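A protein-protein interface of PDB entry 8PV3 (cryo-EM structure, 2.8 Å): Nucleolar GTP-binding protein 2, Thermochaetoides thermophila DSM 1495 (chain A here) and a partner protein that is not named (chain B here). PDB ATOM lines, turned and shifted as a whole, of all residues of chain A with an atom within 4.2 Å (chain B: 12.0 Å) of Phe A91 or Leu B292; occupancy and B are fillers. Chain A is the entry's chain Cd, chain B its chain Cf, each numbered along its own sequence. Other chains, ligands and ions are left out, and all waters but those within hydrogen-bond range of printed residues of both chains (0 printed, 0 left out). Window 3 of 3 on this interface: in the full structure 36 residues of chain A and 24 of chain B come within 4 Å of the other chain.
O of Leu B292 is in hydrogen-bond range of ND2 of Asn A110 (2.9 Å). N of Asn A110 is in hydrogen-bond range of OD1 of Asp B294 (2.9 Å).
SD of Met A95 lies within hydrogen-bond range of NZ of Lys A98. The backbone NH of Leu B292 lies close to the side-chain carboxylate of Asp B290, 3.3 Å away. OD1 of Asp B290 lies within hydrogen-bond range of N of Gly B293, 3.0 Å away. The side-chain carboxylate (OD1) of Asp B290 sits at hydrogen-bond distance from the backbone NH (N) of Asp B294, at 2.5 Å.
Among the printed residues, merely in contact across the chains: Leu A112 with Leu B292 (3.4 Å), Asn A110 with Gly B293 (3.4 Å), Phe A91 with Leu B291 (3.6 Å), Phe A91 with Leu B292 (3.6 Å), Lys A98 with Leu B292 (3.7 Å), Ala A94 with Leu B291 (3.7 Å) and Met A95 with Leu B292 (3.8 Å).
No residue of chain B comes within 4 Å of Thr A87. No residue of chain B comes within 4 Å of Leu A88. No residue of chain B comes within 4 Å of Gln A89. No residue of chain B comes within 4 Å of Ser A90. Of chain B, only Leu B291 (3.6 Å) and Leu B292 (3.6 Å) come within 4 Å of Phe A91. No residue of chain B comes within 4 Å of Glu A93. Of chain B, only Leu B291 comes within 4 Å of Ala A94. Met A95 touches just one residue of chain B: Leu B292. Asn A110 touches just these residues of chain B: Leu B292 (2.9 Å), Gly B293 (3.4 Å) and Asp B294 (2.9 Å). Printed residues of chain A within 4 Å of Leu B291: Phe A91 (3.6 Å) and Ala A94 (3.7 Å). Leu B292 touches just these residues of chain A: Phe A91 (3.6 Å), Met A95 (3.8 Å), Lys A98 (3.7 Å), Asn A110 (2.9 Å) and Leu A112 (3.4 Å). Printed residues of chain A within 4 Å of Gly B293: Asn A110 (3.4 Å). Lys B295 touches none of the printed residues of chain A. Ile B296 touches none of the printed residues of chain A. The nearest residue of chain B that does not touch Phe A91 is Gly B293 (4.7 Å).
Printed residues of chain B that touch a printed residue of chain A: Leu B291, Leu B292, Gly B293 and Asp B294. Hydrophobic or aromatic side chains of chain B that line the printed part of chain A: Leu B291 and Leu B292. Hydrophobic or aromatic side chains of chain A that line the printed part of chain B: Phe A91, Ala A94, Met A95 and Leu A112. Along chain A the printed residues that touch a printed residue of chain B span positions 91 to 112. Among the printed residues, 9 pairs touch across the chains.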
ATOM      1  N   THR A  87      18.713   7.593 -15.892  1.00  0.00           N
ATOM      2  CA  THR A  87      18.703   6.507 -16.868  1.00  0.00           C
ATOM      3  C   THR A  87      17.468   5.632 -16.700  1.00  0.00           C
ATOM      4  O   THR A  87      16.851   5.218 -17.690  1.00  0.00           O
ATOM      5  CB  THR A  87      19.978   5.674 -16.728  1.00  0.00           C
ATOM      6  OG1 THR A  87      21.119   6.537 -16.772  1.00  0.00           O
ATOM      7  CG2 THR A  87      20.088   4.673 -17.858  1.00  0.00           C
ATOM      8  N   LEU A  88      17.083   5.358 -15.449  1.00  0.00           N
ATOM      9  CA  LEU A  88      15.873   4.582 -15.195  1.00  0.00           C
ATOM     10  C   LEU A  88      14.626   5.305 -15.688  1.00  0.00           C
ATOM     11  O   LEU A  88      13.736   4.681 -16.271  1.00  0.00           O
ATOM     12  CB  LEU A  88      15.750   4.265 -13.705  1.00  0.00           C
ATOM     13  CG  LEU A  88      16.512   3.034 -13.220  1.00  0.00           C
ATOM     14  CD1 LEU A  88      16.451   2.929 -11.708  1.00  0.00           C
ATOM     15  CD2 LEU A  88      15.949   1.783 -13.869  1.00  0.00           C
ATOM     16  N   GLN A  89      14.546   6.621 -15.470  1.00  0.00           N
ATOM     17  CA  GLN A  89      13.398   7.388 -15.949  1.00  0.00           C
ATOM     18  C   GLN A  89      13.344   7.425 -17.472  1.00  0.00           C
ATOM     19  O   GLN A  89      12.262   7.333 -18.067  1.00  0.00           O
ATOM     20  CB  GLN A  89      13.441   8.805 -15.382  1.00  0.00           C
ATOM     21  CG  GLN A  89      12.099   9.518 -15.392  1.00  0.00           C
ATOM     22  CD  GLN A  89      10.964   8.638 -14.901  1.00  0.00           C
ATOM     23  OE1 GLN A  89      10.053   8.301 -15.655  1.00  0.00           O
ATOM     24  NE2 GLN A  89      11.012   8.268 -13.626  1.00  0.00           N
ATOM     25  N   SER A  90      14.506   7.560 -18.120  1.00  0.00           N
ATOM     26  CA  SER A  90      14.556   7.535 -19.580  1.00  0.00           C
ATOM     27  C   SER A  90      14.105   6.185 -20.122  1.00  0.00           C
ATOM     28  O   SER A  90      13.380   6.113 -21.122  1.00  0.00           O
ATOM     29  CB  SER A  90      15.970   7.864 -20.058  1.00  0.00           C
ATOM     30  OG  SER A  90      16.386   9.132 -19.583  1.00  0.00           O
ATOM     31  N   PHE A  91      14.513   5.099 -19.462  1.00  0.00           N
ATOM     32  CA  PHE A  91      14.094   3.774 -19.906  1.00  0.00           C
ATOM     33  C   PHE A  91      12.613   3.533 -19.631  1.00  0.00           C
ATOM     34  O   PHE A  91      11.948   2.826 -20.393  1.00  0.00           O
ATOM     35  CB  PHE A  91      14.956   2.702 -19.245  1.00  0.00           C
ATOM     36  CG  PHE A  91      16.271   2.490 -19.928  1.00  0.00           C
ATOM     37  CD1 PHE A  91      16.363   2.546 -21.308  1.00  0.00           C
ATOM     38  CD2 PHE A  91      17.418   2.241 -19.198  1.00  0.00           C
ATOM     39  CE1 PHE A  91      17.569   2.353 -21.945  1.00  0.00           C
ATOM     40  CE2 PHE A  91      18.628   2.049 -19.831  1.00  0.00           C
ATOM     41  CZ  PHE A  91      18.703   2.105 -21.204  1.00  0.00           C
ATOM     42  N   ARG A  92      12.077   4.117 -18.554  1.00  0.00           N
ATOM     43  CA  ARG A  92      10.636   4.051 -18.313  1.00  0.00           C
ATOM     44  C   ARG A  92       9.860   4.764 -19.411  1.00  0.00           C
ATOM     45  O   ARG A  92       8.842   4.254 -19.897  1.00  0.00           O
ATOM     46  CB  ARG A  92      10.293   4.659 -16.954  1.00  0.00           C
ATOM     47  CG  ARG A  92      10.708   3.833 -15.757  1.00  0.00           C
ATOM     48  CD  ARG A  92      10.191   4.442 -14.469  1.00  0.00           C
ATOM     49  NE  ARG A  92      10.714   3.751 -13.296  1.00  0.00           N
ATOM     50  CZ  ARG A  92      11.659   4.234 -12.502  1.00  0.00           C
ATOM     51  NH1 ARG A  92      12.190   5.427 -12.708  1.00  0.00           N
ATOM     52  NH2 ARG A  92      12.081   3.503 -11.476  1.00  0.00           N
ATOM     53  N   GLU A  93      10.333   5.945 -19.817  1.00  0.00           N
ATOM     54  CA  GLU A  93       9.683   6.675 -20.903  1.00  0.00           C
ATOM     55  C   GLU A  93       9.777   5.913 -22.220  1.00  0.00           C
ATOM     56  O   GLU A  93       8.810   5.868 -22.991  1.00  0.00           O
ATOM     57  CB  GLU A  93      10.300   8.066 -21.037  1.00  0.00           C
ATOM     58  CG  GLU A  93       9.805   9.059 -20.002  1.00  0.00           C
ATOM     59  CD  GLU A  93      10.844  10.106 -19.654  1.00  0.00           C
ATOM     60  OE1 GLU A  93      11.683  10.425 -20.521  1.00  0.00           O
ATOM     61  OE2 GLU A  93      10.823  10.609 -18.511  1.00  0.00           O
ATOM     62  N   ALA A  94      10.931   5.296 -22.488  1.00  0.00           N
ATOM     63  CA  ALA A  94      11.088   4.491 -23.698  1.00  0.00           C
ATOM     64  C   ALA A  94      10.172   3.271 -23.685  1.00  0.00           C
ATOM     65  O   ALA A  94       9.588   2.912 -24.715  1.00  0.00           O
ATOM     66  CB  ALA A  94      12.545   4.062 -23.847  1.00  0.00           C
ATOM     67  N   MET A  95      10.039   2.619 -22.528  1.00  0.00           N
ATOM     68  CA  MET A  95       9.172   1.453 -22.413  1.00  0.00           C
ATOM     69  C   MET A  95       7.709   1.850 -22.569  1.00  0.00           C
ATOM     70  O   MET A  95       6.895   1.080 -23.092  1.00  0.00           O
ATOM     71  CB  MET A  95       9.414   0.764 -21.069  1.00  0.00           C
ATOM     72  CG  MET A  95       8.690  -0.556 -20.882  1.00  0.00           C
ATOM     73  SD  MET A  95       9.282  -1.830 -22.009  1.00  0.00           S
ATOM     74  CE  MET A  95       7.860  -2.916 -22.064  1.00  0.00           C
ATOM     75  N   LYS A  98       7.221   2.430 -26.365  1.00  0.00           N
ATOM     76  CA  LYS A  98       7.462   1.288 -27.243  1.00  0.00           C
ATOM     77  C   LYS A  98       6.222   0.943 -28.063  1.00  0.00           C
ATOM     78  O   LYS A  98       5.110   0.872 -27.533  1.00  0.00           O
ATOM     79  CB  LYS A  98       7.891   0.072 -26.421  1.00  0.00           C
ATOM     80  CG  LYS A  98       8.093  -1.191 -27.250  1.00  0.00           C
ATOM     81  CD  LYS A  98       8.283  -2.420 -26.380  1.00  0.00           C
ATOM     82  CE  LYS A  98       9.703  -2.520 -25.871  1.00  0.00           C
ATOM     83  NZ  LYS A  98       9.937  -3.784 -25.119  1.00  0.00           N
ATOM     84  N   ASN A 110      19.190  -6.063 -24.582  1.00  0.00           N
ATOM     85  CA  ASN A 110      20.004  -5.219 -23.720  1.00  0.00           C
ATOM     86  C   ASN A 110      19.799  -5.651 -22.274  1.00  0.00           C
ATOM     87  O   ASN A 110      18.661  -5.717 -21.797  1.00  0.00           O
ATOM     88  CB  ASN A 110      19.645  -3.746 -23.896  1.00  0.00           C
ATOM     89  CG  ASN A 110      20.654  -2.821 -23.252  1.00  0.00           C
ATOM     90  OD1 ASN A 110      21.748  -3.242 -22.880  1.00  0.00           O
ATOM     91  ND2 ASN A 110      20.292  -1.552 -23.118  1.00  0.00           N
ATOM     92  N   LEU A 112      19.201  -5.201 -18.839  1.00  0.00           N
ATOM     93  CA  LEU A 112      18.635  -4.101 -18.079  1.00  0.00           C
ATOM     94  C   LEU A 112      17.925  -4.654 -16.855  1.00  0.00           C
ATOM     95  O   LEU A 112      17.451  -5.795 -16.870  1.00  0.00           O
ATOM     96  CB  LEU A 112      17.651  -3.288 -18.931  1.00  0.00           C
ATOM     97  CG  LEU A 112      18.271  -2.394 -20.003  1.00  0.00           C
ATOM     98  CD1 LEU A 112      17.194  -1.628 -20.744  1.00  0.00           C
ATOM     99  CD2 LEU A 112      19.287  -1.455 -19.388  1.00  0.00           C
ATOM    100  N   ILE A 117      11.970  -1.122 -14.671  1.00  0.00           N
ATOM    101  CA  ILE A 117      11.610  -0.380 -15.868  1.00  0.00           C
ATOM    102  C   ILE A 117      10.176  -0.658 -16.301  1.00  0.00           C
ATOM    103  O   ILE A 117       9.437   0.274 -16.640  1.00  0.00           O
ATOM    104  CB  ILE A 117      12.595  -0.682 -17.021  1.00  0.00           C
ATOM    105  CG1 ILE A 117      14.019  -0.318 -16.604  1.00  0.00           C
ATOM    106  CG2 ILE A 117      12.222   0.078 -18.280  1.00  0.00           C
ATOM    107  CD1 ILE A 117      15.064  -0.716 -17.606  1.00  0.00           C
ATOM    108  N   SER B 288      20.172  -1.191 -36.243  1.00  0.00           N
ATOM    109  CA  SER B 288      19.954   0.005 -35.447  1.00  0.00           C
ATOM    110  C   SER B 288      19.941  -0.367 -33.973  1.00  0.00           C
ATOM    111  O   SER B 288      19.922  -1.541 -33.605  1.00  0.00           O
ATOM    112  CB  SER B 288      18.650   0.707 -35.838  1.00  0.00           C
ATOM    113  OG  SER B 288      17.526  -0.082 -35.495  1.00  0.00           O
ATOM    114  N   MET B 289      19.961   0.658 -33.131  1.00  0.00           N
ATOM    115  CA  MET B 289      19.830   0.516 -31.688  1.00  0.00           C
ATOM    116  C   MET B 289      18.589   1.277 -31.245  1.00  0.00           C
ATOM    117  O   MET B 289      18.478   2.481 -31.494  1.00  0.00           O
ATOM    118  CB  MET B 289      21.078   1.048 -30.981  1.00  0.00           C
ATOM    119  CG  MET B 289      21.028   1.023 -29.467  1.00  0.00           C
ATOM    120  SD  MET B 289      22.201   2.210 -28.782  1.00  0.00           S
ATOM    121  CE  MET B 289      21.634   2.336 -27.091  1.00  0.00           C
ATOM    122  N   ASP B 290      17.656   0.582 -30.598  1.00  0.00           N
ATOM    123  CA  ASP B 290      16.386   1.224 -30.288  1.00  0.00           C
ATOM    124  C   ASP B 290      16.504   2.068 -29.017  1.00  0.00           C
ATOM    125  O   ASP B 290      17.595   2.329 -28.504  1.00  0.00           O
ATOM    126  CB  ASP B 290      15.262   0.191 -30.193  1.00  0.00           C
ATOM    127  CG  ASP B 290      15.400  -0.749 -29.005  1.00  0.00           C
ATOM    128  OD1 ASP B 290      16.482  -0.821 -28.391  1.00  0.00           O
ATOM    129  OD2 ASP B 290      14.403  -1.426 -28.683  1.00  0.00           O
ATOM    130  N   LEU B 291      15.354   2.503 -28.501  1.00  0.00           N
ATOM    131  CA  LEU B 291      15.346   3.372 -27.332  1.00  0.00           C
ATOM    132  C   LEU B 291      15.670   2.630 -26.042  1.00  0.00           C
ATOM    133  O   LEU B 291      16.050   3.270 -25.057  1.00  0.00           O
ATOM    134  CB  LEU B 291      13.991   4.066 -27.211  1.00  0.00           C
ATOM    135  CG  LEU B 291      13.704   5.167 -28.230  1.00  0.00           C
ATOM    136  CD1 LEU B 291      12.316   5.744 -28.014  1.00  0.00           C
ATOM    137  CD2 LEU B 291      14.760   6.256 -28.146  1.00  0.00           C
ATOM    138  N   LEU B 292      15.525   1.306 -26.019  1.00  0.00           N
ATOM    139  CA  LEU B 292      15.875   0.506 -24.853  1.00  0.00           C
ATOM    140  C   LEU B 292      17.256  -0.123 -24.964  1.00  0.00           C
ATOM    141  O   LEU B 292      17.652  -0.881 -24.074  1.00  0.00           O
ATOM    142  CB  LEU B 292      14.830  -0.585 -24.619  1.00  0.00           C
ATOM    143  CG  LEU B 292      13.553  -0.164 -23.896  1.00  0.00           C
ATOM    144  CD1 LEU B 292      12.545  -1.286 -23.934  1.00  0.00           C
ATOM    145  CD2 LEU B 292      13.855   0.221 -22.463  1.00  0.00           C
ATOM    146  N   GLY B 293      17.994   0.169 -26.029  1.00  0.00           N
ATOM    147  CA  GLY B 293      19.315  -0.388 -26.209  1.00  0.00           C
ATOM    148  C   GLY B 293      19.375  -1.702 -26.950  1.00  0.00           C
ATOM    149  O   GLY B 293      20.477  -2.205 -27.191  1.00  0.00           O
ATOM    150  N   ASP B 294      18.233  -2.279 -27.312  1.00  0.00           N
ATOM    151  CA  ASP B 294      18.219  -3.514 -28.078  1.00  0.00           C
ATOM    152  C   ASP B 294      18.700  -3.267 -29.500  1.00  0.00           C
ATOM    153  O   ASP B 294      18.426  -2.223 -30.104  1.00  0.00           O
ATOM    154  CB  ASP B 294      16.813  -4.114 -28.115  1.00  0.00           C
ATOM    155  CG  ASP B 294      16.274  -4.432 -26.737  1.00  0.00           C
ATOM    156  OD1 ASP B 294      17.072  -4.500 -25.783  1.00  0.00           O
ATOM    157  OD2 ASP B 294      15.046  -4.618 -26.610  1.00  0.00           O
ATOM    158  N   LYS B 295      19.427  -4.245 -30.032  1.00  0.00           N
ATOM    159  CA  LYS B 295      19.852  -4.207 -31.422  1.00  0.00           C
ATOM    160  C   LYS B 295      18.719  -4.713 -32.304  1.00  0.00           C
ATOM    161  O   LYS B 295      18.212  -5.822 -32.107  1.00  0.00           O
ATOM    162  CB  LYS B 295      21.108  -5.053 -31.618  1.00  0.00           C
ATOM    163  CG  LYS B 295      21.729  -4.942 -32.994  1.00  0.00           C
ATOM    164  CD  LYS B 295      22.952  -5.830 -33.109  1.00  0.00           C
ATOM    165  CE  LYS B 295      24.035  -5.395 -32.138  1.00  0.00           C
ATOM    166  NZ  LYS B 295      25.217  -6.298 -32.179  1.00  0.00           N
ATOM    167  N   ILE B 296      18.321  -3.896 -33.274  1.00  0.00           N
ATOM    168  CA  ILE B 296      17.139  -4.136 -34.088  1.00  0.00           C
ATOM    169  C   ILE B 296      17.562  -4.277 -35.540  1.00  0.00           C
ATOM    170  O   ILE B 296      18.366  -3.485 -36.045  1.00  0.00           O
ATOM    171  CB  ILE B 296      16.110  -2.998 -33.923  1.00  0.00           C
ATOM    172  CG1 ILE B 296      15.809  -2.756 -32.446  1.00  0.00           C
ATOM    173  CG2 ILE B 296      14.829  -3.320 -34.659  1.00  0.00           C
ATOM    174  CD1 ILE B 296      15.217  -3.955 -31.741  1.00  0.00           C
